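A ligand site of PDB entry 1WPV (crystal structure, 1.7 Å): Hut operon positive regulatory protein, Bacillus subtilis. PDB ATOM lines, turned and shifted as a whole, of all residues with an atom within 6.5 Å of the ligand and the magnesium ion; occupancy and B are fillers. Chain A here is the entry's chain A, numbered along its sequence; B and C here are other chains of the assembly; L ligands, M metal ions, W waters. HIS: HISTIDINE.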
ATOM      1  N   VAL A  85     -16.683  26.482  -6.237  1.00  0.00           N
ATOM      2  CA  VAL A  85     -15.368  26.445  -6.847  1.00  0.00           C
ATOM      3  C   VAL A  85     -14.777  25.039  -6.944  1.00  0.00           C
ATOM      4  O   VAL A  85     -14.192  24.679  -7.955  1.00  0.00           O
ATOM      5  CB  VAL A  85     -14.388  27.359  -6.067  1.00  0.00           C
ATOM      6  CG1 VAL A  85     -12.958  27.062  -6.464  1.00  0.00           C
ATOM      7  CG2 VAL A  85     -14.725  28.828  -6.354  1.00  0.00           C
ATOM      8  N   THR A  86     -14.955  24.239  -5.888  1.00  0.00           N
ATOM      9  CA  THR A  86     -14.399  22.893  -5.864  1.00  0.00           C
ATOM     10  C   THR A  86     -15.336  21.771  -6.348  1.00  0.00           C
ATOM     11  O   THR A  86     -14.866  20.683  -6.715  1.00  0.00           O
ATOM     12  CB  THR A  86     -13.874  22.556  -4.462  1.00  0.00           C
ATOM     13  OG1 THR A  86     -14.936  22.688  -3.515  1.00  0.00           O
ATOM     14  CG2 THR A  86     -12.752  23.518  -4.083  1.00  0.00           C
ATOM     15  N   ARG A  87     -16.630  22.027  -6.358  1.00  0.00           N
ATOM     16  CA  ARG A  87     -17.634  21.070  -6.831  1.00  0.00           C
ATOM     17  C   ARG A  87     -17.453  19.592  -6.435  1.00  0.00           C
ATOM     18  O   ARG A  87     -17.203  18.752  -7.294  1.00  0.00           O
ATOM     19  CB  ARG A  87     -17.745  21.176  -8.360  1.00  0.00           C
ATOM     20  CG  ARG A  87     -18.311  22.516  -8.851  1.00  0.00           C
ATOM     21  CD  ARG A  87     -17.605  22.987 -10.125  1.00  0.00           C
ATOM     22  NE  ARG A  87     -16.196  23.252  -9.841  1.00  0.00           N
ATOM     23  CZ  ARG A  87     -15.172  22.714 -10.495  1.00  0.00           C
ATOM     24  NH1 ARG A  87     -15.388  21.886 -11.513  1.00  0.00           N
ATOM     25  NH2 ARG A  87     -13.930  22.991 -10.113  1.00  0.00           N
ATOM     26  N   LEU A  95      -5.355  17.398  -5.173  1.00  0.00           N
ATOM     27  CA  LEU A  95      -6.032  16.794  -6.314  1.00  0.00           C
ATOM     28  C   LEU A  95      -5.391  17.335  -7.572  1.00  0.00           C
ATOM     29  O   LEU A  95      -5.977  17.331  -8.641  1.00  0.00           O
ATOM     30  CB  LEU A  95      -7.531  17.098  -6.321  1.00  0.00           C
ATOM     31  CG  LEU A  95      -8.334  16.459  -5.184  1.00  0.00           C
ATOM     32  CD1 LEU A  95      -9.817  16.621  -5.471  1.00  0.00           C
ATOM     33  CD2 LEU A  95      -7.983  14.961  -5.068  1.00  0.00           C
ATOM     34  N   LEU A  96      -4.163  17.825  -7.401  1.00  0.00           N
ATOM     35  CA  LEU A  96      -3.374  18.349  -8.497  1.00  0.00           C
ATOM     36  C   LEU A  96      -4.040  19.467  -9.291  1.00  0.00           C
ATOM     37  O   LEU A  96      -4.025  19.467 -10.515  1.00  0.00           O
ATOM     38  CB  LEU A  96      -2.979  17.206  -9.446  1.00  0.00           C
ATOM     39  CG  LEU A  96      -1.767  17.435 -10.347  1.00  0.00           C
ATOM     40  CD1 LEU A  96      -0.536  17.718  -9.500  1.00  0.00           C
ATOM     41  CD2 LEU A  96      -1.551  16.198 -11.227  1.00  0.00           C
ATOM     42  N   ARG A  97      -4.644  20.429  -8.588  1.00  0.00           N
ATOM     43  CA  ARG A  97      -5.253  21.566  -9.261  1.00  0.00           C
ATOM     44  C   ARG A  97      -4.969  22.828  -8.448  1.00  0.00           C
ATOM     45  O   ARG A  97      -4.608  22.746  -7.266  1.00  0.00           O
ATOM     46  CB  ARG A  97      -6.762  21.360  -9.475  1.00  0.00           C
ATOM     47  CG  ARG A  97      -7.584  21.204  -8.228  1.00  0.00           C
ATOM     48  CD  ARG A  97      -9.066  21.039  -8.587  1.00  0.00           C
ATOM     49  NE  ARG A  97      -9.857  20.724  -7.407  1.00  0.00           N
ATOM     50  CZ  ARG A  97     -11.161  20.472  -7.402  1.00  0.00           C
ATOM     51  NH1 ARG A  97     -11.854  20.493  -8.535  1.00  0.00           N
ATOM     52  NH2 ARG A  97     -11.760  20.158  -6.264  1.00  0.00           N
ATOM     53  N   THR A  98      -5.107  23.979  -9.082  1.00  0.00           N
ATOM     54  CA  THR A  98      -4.820  25.238  -8.421  1.00  0.00           C
ATOM     55  C   THR A  98      -5.818  26.288  -8.883  1.00  0.00           C
ATOM     56  O   THR A  98      -6.488  26.114  -9.894  1.00  0.00           O
ATOM     57  CB  THR A  98      -3.373  25.691  -8.757  1.00  0.00           C
ATOM     58  OG1 THR A  98      -3.031  26.860  -8.013  1.00  0.00           O
ATOM     59  CG2 THR A  98      -3.240  25.963 -10.239  1.00  0.00           C
ATOM     60  N   ILE A 128      -9.569  27.590 -12.284  1.00  0.00           N
ATOM     61  CA  ILE A 128      -9.164  26.412 -11.562  1.00  0.00           C
ATOM     62  C   ILE A 128      -8.608  25.498 -12.645  1.00  0.00           C
ATOM     63  O   ILE A 128      -9.207  25.374 -13.713  1.00  0.00           O
ATOM     64  CB  ILE A 128     -10.354  25.733 -10.849  1.00  0.00           C
ATOM     65  CG1 ILE A 128      -9.844  24.608  -9.947  1.00  0.00           C
ATOM     66  CG2 ILE A 128     -11.350  25.187 -11.851  1.00  0.00           C
ATOM     67  CD1 ILE A 128     -10.853  24.173  -8.917  1.00  0.00           C
ATOM     68  N   GLY A 129      -7.454  24.891 -12.394  1.00  0.00           N
ATOM     69  CA  GLY A 129      -6.875  24.010 -13.390  1.00  0.00           C
ATOM     70  C   GLY A 129      -5.603  23.326 -12.924  1.00  0.00           C
ATOM     71  O   GLY A 129      -5.283  23.336 -11.732  1.00  0.00           O
ATOM     72  N   ALA A 130      -4.878  22.724 -13.860  1.00  0.00           N
ATOM     73  CA  ALA A 130      -3.627  22.060 -13.528  1.00  0.00           C
ATOM     74  C   ALA A 130      -2.609  23.125 -13.127  1.00  0.00           C
ATOM     75  O   ALA A 130      -2.814  24.308 -13.404  1.00  0.00           O
ATOM     76  CB  ALA A 130      -3.121  21.275 -14.730  1.00  0.00           C
ATOM     77  N   PRO A 131      -1.511  22.734 -12.475  1.00  0.00           N
ATOM     78  CA  PRO A 131      -0.485  23.699 -12.059  1.00  0.00           C
ATOM     79  C   PRO A 131       0.194  24.373 -13.263  1.00  0.00           C
ATOM     80  O   PRO A 131       1.084  25.198 -13.099  1.00  0.00           O
ATOM     81  CB  PRO A 131       0.493  22.855 -11.253  1.00  0.00           C
ATOM     82  CG  PRO A 131      -0.311  21.649 -10.831  1.00  0.00           C
ATOM     83  CD  PRO A 131      -1.148  21.370 -12.056  1.00  0.00           C
ATOM     84  N   LEU A 135      -3.852  25.544 -18.863  1.00  0.00           N
ATOM     85  CA  LEU A 135      -4.680  24.360 -18.646  1.00  0.00           C
ATOM     86  C   LEU A 135      -5.640  24.623 -17.493  1.00  0.00           C
ATOM     87  O   LEU A 135      -5.390  24.205 -16.360  1.00  0.00           O
ATOM     88  CB  LEU A 135      -3.792  23.153 -18.342  1.00  0.00           C
ATOM     89  CG  LEU A 135      -2.696  22.902 -19.393  1.00  0.00           C
ATOM     90  CD1 LEU A 135      -1.882  21.681 -19.019  1.00  0.00           C
ATOM     91  CD2 LEU A 135      -3.339  22.730 -20.754  1.00  0.00           C
ATOM     92  N   GLU A 136      -6.734  25.305 -17.781  1.00  0.00           N
ATOM     93  CA  GLU A 136      -7.703  25.650 -16.746  1.00  0.00           C
ATOM     94  C   GLU A 136      -8.977  26.227 -17.350  1.00  0.00           C
ATOM     95  O   GLU A 136      -9.031  26.530 -18.543  1.00  0.00           O
ATOM     96  CB  GLU A 136      -7.084  26.690 -15.817  1.00  0.00           C
ATOM     97  CG  GLU A 136      -7.024  28.077 -16.457  1.00  0.00           C
ATOM     98  CD  GLU A 136      -5.640  28.715 -16.395  1.00  0.00           C
ATOM     99  OE1 GLU A 136      -4.696  28.053 -15.906  1.00  0.00           O
ATOM    100  OE2 GLU A 136      -5.505  29.868 -16.847  1.00  0.00           O
ATOM    101  N   HIS A 137     -10.003  26.378 -16.518  1.00  0.00           N
ATOM    102  CA  HIS A 137     -11.249  26.973 -16.955  1.00  0.00           C
ATOM    103  C   HIS A 137     -11.789  27.847 -15.823  1.00  0.00           C
ATOM    104  O   HIS A 137     -11.181  27.907 -14.747  1.00  0.00           O
ATOM    105  CB  HIS A 137     -12.287  25.910 -17.369  1.00  0.00           C
ATOM    106  CG  HIS A 137     -12.651  24.936 -16.301  1.00  0.00           C
ATOM    107  ND1 HIS A 137     -13.254  25.315 -15.119  1.00  0.00           N
ATOM    108  CD2 HIS A 137     -12.556  23.584 -16.254  1.00  0.00           C
ATOM    109  CE1 HIS A 137     -13.512  24.240 -14.396  1.00  0.00           C
ATOM    110  NE2 HIS A 137     -13.102  23.173 -15.064  1.00  0.00           N
ATOM    111  N   GLU B  54      -1.806  10.633 -15.648  1.00  0.00           N
ATOM    112  CA  GLU B  54      -1.769  11.673 -16.679  1.00  0.00           C
ATOM    113  C   GLU B  54      -0.517  11.524 -17.538  1.00  0.00           C
ATOM    114  O   GLU B  54      -0.587  11.479 -18.757  1.00  0.00           O
ATOM    115  CB  GLU B  54      -1.801  13.060 -16.036  1.00  0.00           C
ATOM    116  CG  GLU B  54      -1.311  14.174 -16.965  1.00  0.00           C
ATOM    117  CD  GLU B  54      -1.448  15.556 -16.348  1.00  0.00           C
ATOM    118  OE1 GLU B  54      -1.273  15.702 -15.118  1.00  0.00           O
ATOM    119  OE2 GLU B  54      -1.723  16.513 -17.106  1.00  0.00           O
ATOM    120  N   TYR B  68      -5.834  21.667 -23.660  1.00  0.00           N
ATOM    121  CA  TYR B  68      -6.415  21.375 -22.356  1.00  0.00           C
ATOM    122  C   TYR B  68      -7.582  20.394 -22.429  1.00  0.00           C
ATOM    123  O   TYR B  68      -7.761  19.561 -21.537  1.00  0.00           O
ATOM    124  CB  TYR B  68      -6.877  22.685 -21.720  1.00  0.00           C
ATOM    125  CG  TYR B  68      -7.528  22.542 -20.356  1.00  0.00           C
ATOM    126  CD1 TYR B  68      -6.879  21.875 -19.323  1.00  0.00           C
ATOM    127  CD2 TYR B  68      -8.771  23.112 -20.096  1.00  0.00           C
ATOM    128  CE1 TYR B  68      -7.445  21.778 -18.055  1.00  0.00           C
ATOM    129  CE2 TYR B  68      -9.355  23.025 -18.830  1.00  0.00           C
ATOM    130  CZ  TYR B  68      -8.680  22.358 -17.813  1.00  0.00           C
ATOM    131  OH  TYR B  68      -9.246  22.299 -16.562  1.00  0.00           O
ATOM    132  N   SER B  71      -6.878  16.819 -21.597  1.00  0.00           N
ATOM    133  CA  SER B  71      -6.355  16.688 -20.243  1.00  0.00           C
ATOM    134  C   SER B  71      -7.545  16.859 -19.302  1.00  0.00           C
ATOM    135  O   SER B  71      -7.651  16.196 -18.267  1.00  0.00           O
ATOM    136  CB  SER B  71      -5.307  17.764 -19.959  1.00  0.00           C
ATOM    137  OG  SER B  71      -4.086  17.447 -20.580  1.00  0.00           O
ATOM    138  N   HIS B  72      -8.449  17.748 -19.680  1.00  0.00           N
ATOM    139  CA  HIS B  72      -9.644  18.002 -18.886  1.00  0.00           C
ATOM    140  C   HIS B  72     -10.491  16.736 -18.830  1.00  0.00           C
ATOM    141  O   HIS B  72     -10.950  16.330 -17.769  1.00  0.00           O
ATOM    142  CB  HIS B  72     -10.445  19.159 -19.505  1.00  0.00           C
ATOM    143  CG  HIS B  72     -11.623  19.586 -18.688  1.00  0.00           C
ATOM    144  ND1 HIS B  72     -12.899  19.157 -18.933  1.00  0.00           N
ATOM    145  CD2 HIS B  72     -11.691  20.380 -17.592  1.00  0.00           C
ATOM    146  CE1 HIS B  72     -13.719  19.669 -18.037  1.00  0.00           C
ATOM    147  NE2 HIS B  72     -13.007  20.415 -17.205  1.00  0.00           N
ATOM    148  N   TYR B  75      -8.729  14.218 -16.610  1.00  0.00           N
ATOM    149  CA  TYR B  75      -8.752  14.592 -15.211  1.00  0.00           C
ATOM    150  C   TYR B  75     -10.063  14.196 -14.527  1.00  0.00           C
ATOM    151  O   TYR B  75     -10.055  13.642 -13.418  1.00  0.00           O
ATOM    152  CB  TYR B  75      -8.534  16.096 -15.061  1.00  0.00           C
ATOM    153  CG  TYR B  75      -8.516  16.546 -13.631  1.00  0.00           C
ATOM    154  CD1 TYR B  75      -7.343  16.458 -12.878  1.00  0.00           C
ATOM    155  CD2 TYR B  75      -9.659  17.053 -13.016  1.00  0.00           C
ATOM    156  CE1 TYR B  75      -7.314  16.847 -11.552  1.00  0.00           C
ATOM    157  CE2 TYR B  75      -9.640  17.447 -11.681  1.00  0.00           C
ATOM    158  CZ  TYR B  75      -8.468  17.352 -10.958  1.00  0.00           C
ATOM    159  OH  TYR B  75      -8.435  17.728  -9.633  1.00  0.00           O
ATOM    160  N   HIS B  76     -11.178  14.480 -15.178  1.00  0.00           N
ATOM    161  CA  HIS B  76     -12.476  14.164 -14.609  1.00  0.00           C
ATOM    162  C   HIS B  76     -12.763  12.674 -14.586  1.00  0.00           C
ATOM    163  O   HIS B  76     -13.489  12.195 -13.721  1.00  0.00           O
ATOM    164  CB  HIS B  76     -13.573  14.938 -15.337  1.00  0.00           C
ATOM    165  CG  HIS B  76     -13.693  16.358 -14.887  1.00  0.00           C
ATOM    166  ND1 HIS B  76     -14.139  16.682 -13.625  1.00  0.00           N
ATOM    167  CD2 HIS B  76     -13.331  17.516 -15.467  1.00  0.00           C
ATOM    168  CE1 HIS B  76     -14.059  17.994 -13.456  1.00  0.00           C
ATOM    169  NE2 HIS B  76     -13.566  18.528 -14.565  1.00  0.00           N
ATOM    170  N   GLU C  80     -22.314  20.089 -11.854  1.00  0.00           N
ATOM    171  CA  GLU C  80     -21.336  20.985 -11.257  1.00  0.00           C
ATOM    172  C   GLU C  80     -21.963  22.323 -10.877  1.00  0.00           C
ATOM    173  O   GLU C  80     -21.621  22.892  -9.848  1.00  0.00           O
ATOM    174  CB  GLU C  80     -20.154  21.236 -12.192  1.00  0.00           C
ATOM    175  CG  GLU C  80     -19.377  19.974 -12.566  1.00  0.00           C
ATOM    176  CD  GLU C  80     -17.925  20.259 -12.902  1.00  0.00           C
ATOM    177  OE1 GLU C  80     -17.632  21.381 -13.363  1.00  0.00           O
ATOM    178  N   TRP C 119     -17.094  24.289 -25.480  1.00  0.00           N
ATOM    179  CA  TRP C 119     -17.240  24.044 -24.059  1.00  0.00           C
ATOM    180  C   TRP C 119     -18.627  24.560 -23.732  1.00  0.00           C
ATOM    181  O   TRP C 119     -19.196  25.358 -24.472  1.00  0.00           O
ATOM    182  CB  TRP C 119     -16.195  24.799 -23.239  1.00  0.00           C
ATOM    183  CG  TRP C 119     -14.821  24.238 -23.369  1.00  0.00           C
ATOM    184  CD1 TRP C 119     -14.037  24.235 -24.490  1.00  0.00           C
ATOM    185  CD2 TRP C 119     -14.065  23.592 -22.338  1.00  0.00           C
ATOM    186  NE1 TRP C 119     -12.837  23.610 -24.223  1.00  0.00           N
ATOM    187  CE2 TRP C 119     -12.829  23.212 -22.911  1.00  0.00           C
ATOM    188  CE3 TRP C 119     -14.308  23.287 -20.996  1.00  0.00           C
ATOM    189  CZ2 TRP C 119     -11.841  22.547 -22.182  1.00  0.00           C
ATOM    190  CZ3 TRP C 119     -13.330  22.628 -20.268  1.00  0.00           C
ATOM    191  CH2 TRP C 119     -12.107  22.259 -20.863  1.00  0.00           C
ATOM    192  N   ILE C 144     -18.875  24.158 -15.733  1.00  0.00           N
ATOM    193  CA  ILE C 144     -18.273  24.243 -17.058  1.00  0.00           C
ATOM    194  C   ILE C 144     -17.715  22.896 -17.499  1.00  0.00           C
ATOM    195  O   ILE C 144     -17.079  22.181 -16.714  1.00  0.00           O
ATOM    196  CB  ILE C 144     -17.143  25.306 -17.076  1.00  0.00           C
ATOM    197  CG1 ILE C 144     -17.747  26.689 -16.770  1.00  0.00           C
ATOM    198  CG2 ILE C 144     -16.431  25.319 -18.419  1.00  0.00           C
ATOM    199  CD1 ILE C 144     -16.737  27.819 -16.700  1.00  0.00           C
ATOM    200  N   ASN C 145     -17.948  22.530 -18.752  1.00  0.00           N
ATOM    201  CA  ASN C 145     -17.470  21.251 -19.262  1.00  0.00           C
ATOM    202  C   ASN C 145     -17.139  21.364 -20.746  1.00  0.00           C
ATOM    203  O   ASN C 145     -17.605  22.289 -21.412  1.00  0.00           O
ATOM    204  CB  ASN C 145     -18.547  20.197 -19.043  1.00  0.00           C
ATOM    205  CG  ASN C 145     -18.003  18.769 -19.047  1.00  0.00           C
ATOM    206  OD1 ASN C 145     -16.787  18.542 -19.015  1.00  0.00           O
ATOM    207  ND2 ASN C 145     -18.910  17.803 -19.060  1.00  0.00           N
HETATM  208  CA  HIS L   1     -10.707  20.686 -13.145  1.00  0.00           C
HETATM  209  C   HIS L   1     -11.875  21.157 -12.282  1.00  0.00           C
HETATM  210  O   HIS L   1     -13.016  21.167 -12.783  1.00  0.00           O
HETATM  211  CB  HIS L   1      -9.396  21.315 -12.669  1.00  0.00           C
HETATM  212  CG  HIS L   1      -8.190  20.746 -13.339  1.00  0.00           C
HETATM  213  ND1 HIS L   1      -7.973  20.825 -14.700  1.00  0.00           N
HETATM  214  CD2 HIS L   1      -7.166  20.002 -12.843  1.00  0.00           C
HETATM  215  CE1 HIS L   1      -6.879  20.172 -15.008  1.00  0.00           C
HETATM  216  NE2 HIS L   1      -6.365  19.665 -13.902  1.00  0.00           N
HETATM  217  OXT HIS L   1     -11.652  21.493 -11.103  1.00  0.00           O
HETATM  218 MG    MG M   1     -13.259  20.809 -14.978  1.00  0.00          MG
HETATM  219  O   HOH W   1      -3.708  18.258 -12.826  1.00  0.00           O
HETATM  220  O   HOH W   2     -15.609  20.875 -15.105  1.00  0.00           O
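Water W2 lies within hydrogen-bond range of O of Ile 144 of chain C (2.5 Å) and OE1 of Glu 80 of chain C (2.7 Å).
Water W1 lies within hydrogen-bond range of the backbone carbonyl oxygen of Leu 96 (2.6 Å) and a nitrogen (NE2) of the ligand (3.2 Å).
The backbone carbonyl oxygen (O) of His 137 sits at hydrogen-bond distance from the backbone NH (N) of Ile 128 (3.0 Å).
O of Thr 86 is in hydrogen-bond range of NH2 of Arg 97, 3.2 Å away.
OE1 of Glu 80 of chain C lies within salt-bridge range of NH1 of Arg 87.
The backbone carbonyl oxygen (O) of Val 85 lies within hydrogen-bond range of the guanidinium group (NH2) of Arg 87.
The backbone NH (N) of Ala 130 lies within hydrogen-bond range of the backbone carbonyl oxygen (O) of Leu 135 (3.0 Å).
The side-chain hydroxyl (OH) of Tyr 75 of chain B lies within hydrogen-bond range of the backbone carbonyl oxygen (O) of Leu 95.
The backbone carbonyl oxygen (O) of Gly 129 is in hydrogen-bond range of the backbone NH (N) of Thr 98 (2.7 Å).
The side-chain hydroxyl (OH) of Tyr 68 of chain B lies within hydrogen-bond range of a nitrogen (ND1) of the ligand (2.7 Å).
NH1 of Arg 97 is in salt-bridge range of OXT of the ligand (2.8 Å).
NH2 of Arg 87 lies within salt-bridge range of OXT of the ligand, at 2.9 Å.
The backbone NH (N) of Ala 130 sits close to a nitrogen (NE2) of the ligand.
O of the ligand is bound to the magnesium ion, at 2.2 Å.
The magnesium ion is bound by a ring nitrogen (NE2) of His 72 of chain B.
The magnesium ion is bound by a ring nitrogen (NE2) of His 76 of chain B, at 2.3 Å.
The magnesium ion is bound by water W2.
NE2 of His 137 binds the magnesium ion (2.4 Å).
Leu 96 touches the ligand (O to CD2, 3.9 Å).
Ile 128 touches the ligand (CD1 to OXT, 3.5 Å).
CA of Gly 129 touches CG of the ligand (3.5 Å).
Tyr 75 of chain B touches the ligand.
Of the 24 residues printed, 10 come within 4 Å of the ligand.
The nearest printed residue that does not touch the ligand is His 72 of chain B (4.5 Å).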
